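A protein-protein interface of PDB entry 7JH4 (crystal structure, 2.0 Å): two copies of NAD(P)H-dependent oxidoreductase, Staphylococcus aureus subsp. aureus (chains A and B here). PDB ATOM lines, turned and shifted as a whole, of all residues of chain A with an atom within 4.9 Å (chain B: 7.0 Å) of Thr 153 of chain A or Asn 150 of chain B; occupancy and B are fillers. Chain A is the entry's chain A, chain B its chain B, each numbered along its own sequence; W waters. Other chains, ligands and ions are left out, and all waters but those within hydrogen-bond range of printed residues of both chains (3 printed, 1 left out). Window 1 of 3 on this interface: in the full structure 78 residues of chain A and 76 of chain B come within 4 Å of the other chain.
OD1 of Asn 150 of chain B sits close to O of Gly 149 of chain A, 3.3 Å away. The backbone carbonyl oxygen (O) of Gly 149 of chain B sits close to the side-chain amide oxygen (OD1) of Asn 150 of chain A, at 3.3 Å. OG1 of Thr 153 of chain B lies within hydrogen-bond range of OD1 of Asn 150 of chain A. The side-chain amide oxygen of Asn 150 of chain B lies within hydrogen-bond range of the side-chain hydroxyl of Thr 153 of chain A (2.5 Å).
The side-chain hydroxyl of Thr 153 of chain A lies within hydrogen-bond range of the backbone carbonyl oxygen of Gly 149 of chain A, at 3.1 Å. O of Ser 38 of chain B is in hydrogen-bond range of OG of Ser 42 of chain B, at 2.8 Å. OG1 of Thr 154 of chain B sits close to OG of Ser 38 of chain B (3.4 Å). The side-chain hydroxyl (OG) of Ser 42 of chain B sits at hydrogen-bond distance from the side-chain amide nitrogen (ND2) of Asn 150 of chain B (2.9 Å). The backbone carbonyl oxygen (O) of Gly 149 of chain B lies within hydrogen-bond range of the side-chain hydroxyl (OG1) of Thr 153 of chain B, 3.3 Å away. OG1 of Thr 154 of chain B lies within hydrogen-bond range of O of Asn 150 of chain B.
CE2 of Phe 12 of chain A touches O of Ser 38 of chain B (3.3 Å). Asn 150 of chain B touches Phe 12 of chain A (ND2 to CE2, 3.5 Å). Phe 12 of chain A touches Thr 154 of chain B (CE1 to OG1, 3.6 Å). Gly 149 of chain A touches Ile 146 of chain B. CG of Asn 150 of chain A touches CZ of Phe 12 of chain B, at 3.6 Å. Pro 43 of chain B touches Met 152 of chain A (CG to CE, 3.6 Å). Ile 8 of chain B touches Thr 154 of chain A (CG2 to OG1, 3.7 Å). Phe 12 of chain B touches Thr 154 of chain A. Leu 157 of chain A touches Ile 8 of chain B (CB to CD1, 3.8 Å). CD1 of Leu 157 of chain B touches CD1 of Leu 157 of chain A (3.9 Å).
Printed residues of chain B within 4 Å of Asn 150 of chain A: Phe 12, Gly 149 and Thr 153. Of chain B, only Asn 150 (2.5 Å) comes within 4 Å of Thr 153 of chain A. Of the printed residues of chain B, Thr 154 of chain A touches Ile 8 and Phe 12. Of the printed residues of chain A, Ile 8 of chain B touches Thr 154 (3.7 Å) and Leu 157 (3.8 Å). Ser 42 of chain B touches none of the printed residues of chain A. Ala 147 of chain B touches none of the printed residues of chain A. Of the printed residues of chain A, Gly 149 of chain B touches Asn 150. Of chain A, only Phe 12, Gly 149 and Thr 153 come within 4 Å of Asn 150 of chain B. Printed residues of chain A within 4 Å of Leu 157 of chain B: Leu 157. The nearest residue of chain A that does not touch Asn 150 of chain B is Asn 150 of chain A (4.3 Å).
Of the 10 printed residues of chain A, 7 touch a printed residue of chain B. Hydrophobic or aromatic side chains of chain A that line the printed part of chain B: Phe 12, Met 152 and Leu 157. Along chain A the printed residues that touch a printed residue of chain B span positions 12 to 157. Hydrophobic or aromatic side chains of chain B that line the printed part of chain A: Ile 8, Phe 12, Pro 43, Ile 146 and Leu 157. Among the printed residues, 14 pairs touch across the chains. Among the printed residues, no Asp or Glu carboxylate lies within 4 Å of a Lys or Arg side-chain nitrogen of the other chain.
Phe 12 of chain A touches Asn 150 of chain B, and with the chains exchanged Asn 150 of chain A touches Phe 12 of chain B. Phe 12 of chain A touches Thr 154 of chain B, and with the chains exchanged Thr 154 of chain A touches Phe 12 of chain B. Asn 150 of chain A touches Thr 153 of chain B, and with the chains exchanged Thr 153 of chain A touches Asn 150 of chain B. Leu 157 of chain A touches its own counterpart, Leu 157 of chain B. Of the 14 pairs that touch across the chains among the printed residues, 9 have their exchanged pair printed and touching as well.
Water W2 bridges the backbone carbonyl oxygen (O) of Leu 41 of chain B (2.7 Å) and the backbone carbonyl oxygen (O) of Phe 12 of chain A (2.7 Å). Water W3 lies within hydrogen-bond range of the side-chain amide nitrogen of Asn 150 of chain B (3.0 Å), the side-chain hydroxyl of Thr 153 of chain A (3.2 Å) and the backbone carbonyl oxygen of Gly 149 of chain A (3.4 Å). Water W1 lies within hydrogen-bond range of ND2 of Asn 150 of chain A (3.0 Å), O of Gly 149 of chain B (3.2 Å) and OG1 of Thr 153 of chain B (3.3 Å).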
ATOM      1  N   PHE A  12      -4.175   2.235 -27.310  1.00  0.00           N
ATOM      2  CA  PHE A  12      -3.292   2.732 -26.258  1.00  0.00           C
ATOM      3  C   PHE A  12      -3.097   4.245 -26.333  1.00  0.00           C
ATOM      4  O   PHE A  12      -2.674   4.851 -25.341  1.00  0.00           O
ATOM      5  CB  PHE A  12      -1.933   2.030 -26.298  1.00  0.00           C
ATOM      6  CG  PHE A  12      -1.922   0.706 -25.592  1.00  0.00           C
ATOM      7  CD1 PHE A  12      -2.512  -0.409 -26.176  1.00  0.00           C
ATOM      8  CD2 PHE A  12      -1.340   0.579 -24.334  1.00  0.00           C
ATOM      9  CE1 PHE A  12      -2.520  -1.631 -25.527  1.00  0.00           C
ATOM     10  CE2 PHE A  12      -1.345  -0.638 -23.679  1.00  0.00           C
ATOM     11  CZ  PHE A  12      -1.936  -1.748 -24.280  1.00  0.00           C
ATOM     12  N   GLY A 149      -5.088  -2.985 -15.620  1.00  0.00           N
ATOM     13  CA  GLY A 149      -4.627  -2.685 -16.970  1.00  0.00           C
ATOM     14  C   GLY A 149      -5.471  -3.358 -18.040  1.00  0.00           C
ATOM     15  O   GLY A 149      -5.817  -2.737 -19.050  1.00  0.00           O
ATOM     16  N   ASN A 150      -5.828  -4.636 -17.830  1.00  0.00           N
ATOM     17  CA  ASN A 150      -6.614  -5.357 -18.832  1.00  0.00           C
ATOM     18  C   ASN A 150      -7.985  -4.720 -19.018  1.00  0.00           C
ATOM     19  O   ASN A 150      -8.486  -4.619 -20.144  1.00  0.00           O
ATOM     20  CB  ASN A 150      -6.767  -6.832 -18.444  1.00  0.00           C
ATOM     21  CG  ASN A 150      -5.525  -7.650 -18.753  1.00  0.00           C
ATOM     22  OD1 ASN A 150      -4.719  -7.273 -19.610  1.00  0.00           O
ATOM     23  ND2 ASN A 150      -5.358  -8.774 -18.052  1.00  0.00           N
ATOM     24  N   MET A 151      -8.615  -4.293 -17.920  1.00  0.00           N
ATOM     25  CA  MET A 151      -9.940  -3.684 -18.009  1.00  0.00           C
ATOM     26  C   MET A 151      -9.902  -2.355 -18.754  1.00  0.00           C
ATOM     27  O   MET A 151     -10.770  -2.079 -19.585  1.00  0.00           O
ATOM     28  CB  MET A 151     -10.530  -3.501 -16.601  1.00  0.00           C
ATOM     29  CG  MET A 151     -10.776  -4.839 -15.914  1.00  0.00           C
ATOM     30  SD  MET A 151     -11.328  -4.652 -14.212  1.00  0.00           S
ATOM     31  CE  MET A 151     -12.951  -3.934 -14.462  1.00  0.00           C
ATOM     32  N   MET A 152      -8.929  -1.501 -18.454  1.00  0.00           N
ATOM     33  CA  MET A 152      -8.838  -0.226 -19.164  1.00  0.00           C
ATOM     34  C   MET A 152      -8.543  -0.439 -20.644  1.00  0.00           C
ATOM     35  O   MET A 152      -9.126   0.228 -21.506  1.00  0.00           O
ATOM     36  CB  MET A 152      -7.761   0.648 -18.514  1.00  0.00           C
ATOM     37  CG  MET A 152      -8.102   1.109 -17.115  1.00  0.00           C
ATOM     38  SD  MET A 152      -6.837   2.204 -16.478  1.00  0.00           S
ATOM     39  CE  MET A 152      -5.412   1.109 -16.378  1.00  0.00           C
ATOM     40  N   THR A 153      -7.658  -1.377 -20.964  1.00  0.00           N
ATOM     41  CA  THR A 153      -7.321  -1.628 -22.363  1.00  0.00           C
ATOM     42  C   THR A 153      -8.505  -2.202 -23.124  1.00  0.00           C
ATOM     43  O   THR A 153      -8.782  -1.796 -24.264  1.00  0.00           O
ATOM     44  CB  THR A 153      -6.125  -2.566 -22.447  1.00  0.00           C
ATOM     45  OG1 THR A 153      -4.985  -1.905 -21.896  1.00  0.00           O
ATOM     46  CG2 THR A 153      -5.843  -2.980 -23.896  1.00  0.00           C
ATOM     47  N   THR A 154      -9.191  -3.177 -22.528  1.00  0.00           N
ATOM     48  CA  THR A 154     -10.411  -3.701 -23.130  1.00  0.00           C
ATOM     49  C   THR A 154     -11.396  -2.570 -23.389  1.00  0.00           C
ATOM     50  O   THR A 154     -12.001  -2.485 -24.463  1.00  0.00           O
ATOM     51  CB  THR A 154     -11.036  -4.754 -22.206  1.00  0.00           C
ATOM     52  OG1 THR A 154     -10.173  -5.894 -22.092  1.00  0.00           O
ATOM     53  CG2 THR A 154     -12.392  -5.200 -22.731  1.00  0.00           C
ATOM     54  N   ALA A 155     -11.575  -1.684 -22.399  1.00  0.00           N
ATOM     55  CA  ALA A 155     -12.507  -0.578 -22.583  1.00  0.00           C
ATOM     56  C   ALA A 155     -12.076   0.284 -23.755  1.00  0.00           C
ATOM     57  O   ALA A 155     -12.892   0.639 -24.616  1.00  0.00           O
ATOM     58  CB  ALA A 155     -12.621   0.261 -21.307  1.00  0.00           C
ATOM     59  N   ALA A 156     -10.790   0.601 -23.828  1.00  0.00           N
ATOM     60  CA  ALA A 156     -10.310   1.440 -24.919  1.00  0.00           C
ATOM     61  C   ALA A 156     -10.614   0.794 -26.264  1.00  0.00           C
ATOM     62  O   ALA A 156     -11.116   1.451 -27.183  1.00  0.00           O
ATOM     63  CB  ALA A 156      -8.812   1.698 -24.758  1.00  0.00           C
ATOM     64  N   LEU A 157     -10.353  -0.510 -26.387  1.00  0.00           N
ATOM     65  CA  LEU A 157     -10.585  -1.182 -27.666  1.00  0.00           C
ATOM     66  C   LEU A 157     -12.047  -1.116 -28.077  1.00  0.00           C
ATOM     67  O   LEU A 157     -12.361  -1.240 -29.259  1.00  0.00           O
ATOM     68  CB  LEU A 157     -10.124  -2.639 -27.610  1.00  0.00           C
ATOM     69  CG  LEU A 157      -8.607  -2.823 -27.676  1.00  0.00           C
ATOM     70  CD1 LEU A 157      -8.186  -4.069 -26.911  1.00  0.00           C
ATOM     71  CD2 LEU A 157      -8.137  -2.879 -29.129  1.00  0.00           C
ATOM     72  N   ILE B   8     -11.881  -9.440 -28.436  1.00  0.00           N
ATOM     73  CA  ILE B   8     -11.238  -9.290 -27.132  1.00  0.00           C
ATOM     74  C   ILE B   8     -11.405 -10.567 -26.322  1.00  0.00           C
ATOM     75  O   ILE B   8     -10.435 -11.105 -25.776  1.00  0.00           O
ATOM     76  CB  ILE B   8     -11.788  -8.060 -26.385  1.00  0.00           C
ATOM     77  CG1 ILE B   8     -11.546  -6.791 -27.210  1.00  0.00           C
ATOM     78  CG2 ILE B   8     -11.127  -7.918 -25.011  1.00  0.00           C
ATOM     79  CD1 ILE B   8     -12.294  -5.563 -26.709  1.00  0.00           C
ATOM     80  N   PHE B  12      -8.474 -13.150 -24.697  1.00  0.00           N
ATOM     81  CA  PHE B  12      -8.343 -13.474 -23.284  1.00  0.00           C
ATOM     82  C   PHE B  12      -8.498 -14.968 -23.029  1.00  0.00           C
ATOM     83  O   PHE B  12      -8.033 -15.462 -21.997  1.00  0.00           O
ATOM     84  CB  PHE B  12      -9.358 -12.681 -22.462  1.00  0.00           C
ATOM     85  CG  PHE B  12      -8.846 -11.345 -22.019  1.00  0.00           C
ATOM     86  CD1 PHE B  12      -8.790 -10.275 -22.905  1.00  0.00           C
ATOM     87  CD2 PHE B  12      -8.387 -11.168 -20.723  1.00  0.00           C
ATOM     88  CE1 PHE B  12      -8.292  -9.039 -22.500  1.00  0.00           C
ATOM     89  CE2 PHE B  12      -7.887  -9.948 -20.308  1.00  0.00           C
ATOM     90  CZ  PHE B  12      -7.836  -8.878 -21.202  1.00  0.00           C
ATOM     91  N   THR B  34       5.235  -3.604 -31.191  1.00  0.00           N
ATOM     92  CA  THR B  34       3.883  -3.338 -30.685  1.00  0.00           C
ATOM     93  C   THR B  34       3.737  -3.792 -29.238  1.00  0.00           C
ATOM     94  O   THR B  34       3.178  -3.075 -28.400  1.00  0.00           O
ATOM     95  CB  THR B  34       2.835  -4.040 -31.560  1.00  0.00           C
ATOM     96  OG1 THR B  34       2.987  -3.642 -32.920  1.00  0.00           O
ATOM     97  CG2 THR B  34       1.420  -3.695 -31.094  1.00  0.00           C
ATOM     98  N   ILE B  35       4.219  -4.997 -28.932  1.00  0.00           N
ATOM     99  CA  ILE B  35       4.190  -5.493 -27.557  1.00  0.00           C
ATOM    100  C   ILE B  35       4.943  -4.542 -26.626  1.00  0.00           C
ATOM    101  O   ILE B  35       4.459  -4.193 -25.541  1.00  0.00           O
ATOM    102  CB  ILE B  35       4.760  -6.927 -27.502  1.00  0.00           C
ATOM    103  CG1 ILE B  35       3.861  -7.886 -28.290  1.00  0.00           C
ATOM    104  CG2 ILE B  35       4.895  -7.404 -26.066  1.00  0.00           C
ATOM    105  CD1 ILE B  35       4.524  -9.220 -28.583  1.00  0.00           C
ATOM    106  N   SER B  38       3.084  -1.358 -25.969  1.00  0.00           N
ATOM    107  CA  SER B  38       1.996  -1.463 -25.000  1.00  0.00           C
ATOM    108  C   SER B  38       2.516  -1.287 -23.576  1.00  0.00           C
ATOM    109  O   SER B  38       1.803  -0.770 -22.714  1.00  0.00           O
ATOM    110  CB  SER B  38       1.269  -2.802 -25.142  1.00  0.00           C
ATOM    111  OG  SER B  38       2.044  -3.886 -24.654  1.00  0.00           O
ATOM    112  N   GLY B  39       3.754  -1.705 -23.308  1.00  0.00           N
ATOM    113  CA  GLY B  39       4.337  -1.422 -22.004  1.00  0.00           C
ATOM    114  C   GLY B  39       4.667   0.046 -21.836  1.00  0.00           C
ATOM    115  O   GLY B  39       4.267   0.678 -20.849  1.00  0.00           O
ATOM    116  N   LEU B  41       3.480   2.691 -23.221  1.00  0.00           N
ATOM    117  CA  LEU B  41       2.332   3.583 -23.204  1.00  0.00           C
ATOM    118  C   LEU B  41       1.364   3.260 -22.070  1.00  0.00           C
ATOM    119  O   LEU B  41       0.262   3.824 -22.024  1.00  0.00           O
ATOM    120  CB  LEU B  41       1.601   3.522 -24.543  1.00  0.00           C
ATOM    121  CG  LEU B  41       2.474   3.865 -25.767  1.00  0.00           C
ATOM    122  CD1 LEU B  41       1.765   3.460 -27.053  1.00  0.00           C
ATOM    123  CD2 LEU B  41       2.813   5.344 -25.773  1.00  0.00           C
ATOM    124  N   SER B  42       1.729   2.336 -21.190  1.00  0.00           N
ATOM    125  CA  SER B  42       0.850   1.997 -20.090  1.00  0.00           C
ATOM    126  C   SER B  42       0.713   3.189 -19.153  1.00  0.00           C
ATOM    127  O   SER B  42       1.660   3.957 -18.964  1.00  0.00           O
ATOM    128  CB  SER B  42       1.380   0.803 -19.305  1.00  0.00           C
ATOM    129  OG  SER B  42       1.185  -0.386 -20.044  1.00  0.00           O
ATOM    130  N   PRO B  43      -0.461   3.368 -18.552  1.00  0.00           N
ATOM    131  CA  PRO B  43      -0.617   4.419 -17.543  1.00  0.00           C
ATOM    132  C   PRO B  43       0.150   4.057 -16.284  1.00  0.00           C
ATOM    133  O   PRO B  43       0.477   2.895 -16.046  1.00  0.00           O
ATOM    134  CB  PRO B  43      -2.124   4.438 -17.297  1.00  0.00           C
ATOM    135  CG  PRO B  43      -2.544   3.009 -17.499  1.00  0.00           C
ATOM    136  CD  PRO B  43      -1.678   2.544 -18.684  1.00  0.00           C
ATOM    137  N   THR B 144       4.163  -1.667 -12.556  1.00  0.00           N
ATOM    138  CA  THR B 144       4.736  -2.499 -13.607  1.00  0.00           C
ATOM    139  C   THR B 144       3.794  -3.624 -13.993  1.00  0.00           C
ATOM    140  O   THR B 144       3.836  -4.090 -15.141  1.00  0.00           O
ATOM    141  CB  THR B 144       6.116  -3.063 -13.196  1.00  0.00           C
ATOM    142  OG1 THR B 144       5.997  -4.005 -12.113  1.00  0.00           O
ATOM    143  CG2 THR B 144       7.024  -1.939 -12.783  1.00  0.00           C
ATOM    144  N   TYR B 145       2.922  -4.060 -13.069  1.00  0.00           N
ATOM    145  CA  TYR B 145       1.971  -5.122 -13.403  1.00  0.00           C
ATOM    146  C   TYR B 145       0.872  -4.632 -14.331  1.00  0.00           C
ATOM    147  O   TYR B 145       0.274  -5.449 -15.038  1.00  0.00           O
ATOM    148  CB  TYR B 145       1.353  -5.740 -12.135  1.00  0.00           C
ATOM    149  CG  TYR B 145       2.270  -6.743 -11.421  1.00  0.00           C
ATOM    150  CD1 TYR B 145       3.551  -6.388 -11.035  1.00  0.00           C
ATOM    151  CD2 TYR B 145       1.852  -8.043 -11.156  1.00  0.00           C
ATOM    152  CE1 TYR B 145       4.383  -7.278 -10.389  1.00  0.00           C
ATOM    153  CE2 TYR B 145       2.682  -8.947 -10.517  1.00  0.00           C
ATOM    154  CZ  TYR B 145       3.950  -8.555 -10.131  1.00  0.00           C
ATOM    155  OH  TYR B 145       4.803  -9.425  -9.488  1.00  0.00           O
ATOM    156  N   ILE B 146       0.585  -3.328 -14.351  1.00  0.00           N
ATOM    157  CA  ILE B 146      -0.257  -2.787 -15.411  1.00  0.00           C
ATOM    158  C   ILE B 146       0.402  -3.039 -16.762  1.00  0.00           C
ATOM    159  O   ILE B 146      -0.210  -3.588 -17.685  1.00  0.00           O
ATOM    160  CB  ILE B 146      -0.526  -1.285 -15.189  1.00  0.00           C
ATOM    161  CG1 ILE B 146      -1.220  -1.037 -13.847  1.00  0.00           C
ATOM    162  CG2 ILE B 146      -1.363  -0.714 -16.354  1.00  0.00           C
ATOM    163  CD1 ILE B 146      -1.223   0.436 -13.407  1.00  0.00           C
ATOM    164  N   ALA B 147       1.673  -2.657 -16.888  1.00  0.00           N
ATOM    165  CA  ALA B 147       2.387  -2.875 -18.143  1.00  0.00           C
ATOM    166  C   ALA B 147       2.481  -4.364 -18.477  1.00  0.00           C
ATOM    167  O   ALA B 147       2.321  -4.761 -19.643  1.00  0.00           O
ATOM    168  CB  ALA B 147       3.775  -2.239 -18.062  1.00  0.00           C
ATOM    169  N   LEU B 148       2.722  -5.202 -17.465  1.00  0.00           N
ATOM    170  CA  LEU B 148       2.722  -6.652 -17.660  1.00  0.00           C
ATOM    171  C   LEU B 148       1.413  -7.130 -18.290  1.00  0.00           C
ATOM    172  O   LEU B 148       1.409  -7.779 -19.336  1.00  0.00           O
ATOM    173  CB  LEU B 148       2.965  -7.347 -16.318  1.00  0.00           C
ATOM    174  CG  LEU B 148       2.935  -8.874 -16.344  1.00  0.00           C
ATOM    175  CD1 LEU B 148       4.121  -9.405 -17.142  1.00  0.00           C
ATOM    176  CD2 LEU B 148       2.917  -9.429 -14.941  1.00  0.00           C
ATOM    177  N   GLY B 149       0.278  -6.818 -17.672  1.00  0.00           N
ATOM    178  CA  GLY B 149      -0.989  -7.242 -18.252  1.00  0.00           C
ATOM    179  C   GLY B 149      -1.162  -6.736 -19.672  1.00  0.00           C
ATOM    180  O   GLY B 149      -1.589  -7.474 -20.557  1.00  0.00           O
ATOM    181  N   ASN B 150      -0.795  -5.474 -19.912  1.00  0.00           N
ATOM    182  CA  ASN B 150      -0.998  -4.877 -21.225  1.00  0.00           C
ATOM    183  C   ASN B 150      -0.174  -5.578 -22.286  1.00  0.00           C
ATOM    184  O   ASN B 150      -0.663  -5.814 -23.397  1.00  0.00           O
ATOM    185  CB  ASN B 150      -0.658  -3.389 -21.188  1.00  0.00           C
ATOM    186  CG  ASN B 150      -1.830  -2.539 -20.724  1.00  0.00           C
ATOM    187  OD1 ASN B 150      -2.990  -2.952 -20.824  1.00  0.00           O
ATOM    188  ND2 ASN B 150      -1.533  -1.334 -20.235  1.00  0.00           N
ATOM    189  N   MET B 151       1.077  -5.932 -21.966  1.00  0.00           N
ATOM    190  CA  MET B 151       1.922  -6.603 -22.955  1.00  0.00           C
ATOM    191  C   MET B 151       1.431  -8.014 -23.256  1.00  0.00           C
ATOM    192  O   MET B 151       1.492  -8.461 -24.409  1.00  0.00           O
ATOM    193  CB  MET B 151       3.377  -6.630 -22.475  1.00  0.00           C
ATOM    194  CG  MET B 151       3.964  -5.245 -22.256  1.00  0.00           C
ATOM    195  SD  MET B 151       5.524  -5.332 -21.343  1.00  0.00           S
ATOM    196  CE  MET B 151       6.593  -6.042 -22.574  1.00  0.00           C
ATOM    197  N   MET B 152       0.955  -8.744 -22.238  1.00  0.00           N
ATOM    198  CA  MET B 152       0.413 -10.083 -22.492  1.00  0.00           C
ATOM    199  C   MET B 152      -0.864 -10.030 -23.324  1.00  0.00           C
ATOM    200  O   MET B 152      -1.047 -10.845 -24.239  1.00  0.00           O
ATOM    201  CB  MET B 152       0.150 -10.811 -21.176  1.00  0.00           C
ATOM    202  CG  MET B 152       1.405 -11.173 -20.417  1.00  0.00           C
ATOM    203  SD  MET B 152       1.021 -12.113 -18.929  1.00  0.00           S
ATOM    204  CE  MET B 152       0.152 -10.942 -17.901  1.00  0.00           C
ATOM    205  N   THR B 153      -1.765  -9.096 -23.014  1.00  0.00           N
ATOM    206  CA  THR B 153      -2.989  -8.963 -23.796  1.00  0.00           C
ATOM    207  C   THR B 153      -2.675  -8.517 -25.212  1.00  0.00           C
ATOM    208  O   THR B 153      -3.244  -9.042 -26.181  1.00  0.00           O
ATOM    209  CB  THR B 153      -3.943  -7.973 -23.141  1.00  0.00           C
ATOM    210  OG1 THR B 153      -4.422  -8.525 -21.915  1.00  0.00           O
ATOM    211  CG2 THR B 153      -5.135  -7.720 -24.033  1.00  0.00           C
ATOM    212  N   THR B 154      -1.766  -7.553 -25.348  1.00  0.00           N
ATOM    213  CA  THR B 154      -1.367  -7.106 -26.673  1.00  0.00           C
ATOM    214  C   THR B 154      -0.840  -8.272 -27.493  1.00  0.00           C
ATOM    215  O   THR B 154      -1.285  -8.508 -28.619  1.00  0.00           O
ATOM    216  CB  THR B 154      -0.316  -5.999 -26.554  1.00  0.00           C
ATOM    217  OG1 THR B 154      -0.935  -4.836 -25.999  1.00  0.00           O
ATOM    218  CG2 THR B 154       0.242  -5.640 -27.921  1.00  0.00           C
ATOM    219  N   ALA B 155       0.106  -9.024 -26.937  1.00  0.00           N
ATOM    220  CA  ALA B 155       0.608 -10.182 -27.658  1.00  0.00           C
ATOM    221  C   ALA B 155      -0.530 -11.120 -28.047  1.00  0.00           C
ATOM    222  O   ALA B 155      -0.594 -11.583 -29.190  1.00  0.00           O
ATOM    223  CB  ALA B 155       1.665 -10.907 -26.824  1.00  0.00           C
ATOM    224  N   ALA B 156      -1.461 -11.383 -27.129  1.00  0.00           N
ATOM    225  CA  ALA B 156      -2.529 -12.335 -27.429  1.00  0.00           C
ATOM    226  C   ALA B 156      -3.395 -11.847 -28.586  1.00  0.00           C
ATOM    227  O   ALA B 156      -3.781 -12.633 -29.460  1.00  0.00           O
ATOM    228  CB  ALA B 156      -3.380 -12.586 -26.188  1.00  0.00           C
ATOM    229  N   LEU B 157      -3.725 -10.554 -28.598  1.00  0.00           N
ATOM    230  CA  LEU B 157      -4.460  -9.991 -29.720  1.00  0.00           C
ATOM    231  C   LEU B 157      -3.710 -10.201 -31.027  1.00  0.00           C
ATOM    232  O   LEU B 157      -4.325 -10.219 -32.100  1.00  0.00           O
ATOM    233  CB  LEU B 157      -4.719  -8.505 -29.490  1.00  0.00           C
ATOM    234  CG  LEU B 157      -5.773  -8.268 -28.410  1.00  0.00           C
ATOM    235  CD1 LEU B 157      -5.579  -6.911 -27.760  1.00  0.00           C
ATOM    236  CD2 LEU B 157      -7.178  -8.386 -29.010  1.00  0.00           C
HETATM  237  O   HOH W   1      -2.998 -10.105 -19.365  1.00  0.00           O
HETATM  238  O   HOH W   2      -2.321   3.767 -22.857  1.00  0.00           O
HETATM  239  O   HOH W   3      -4.079   0.110 -19.528  1.00  0.00           O
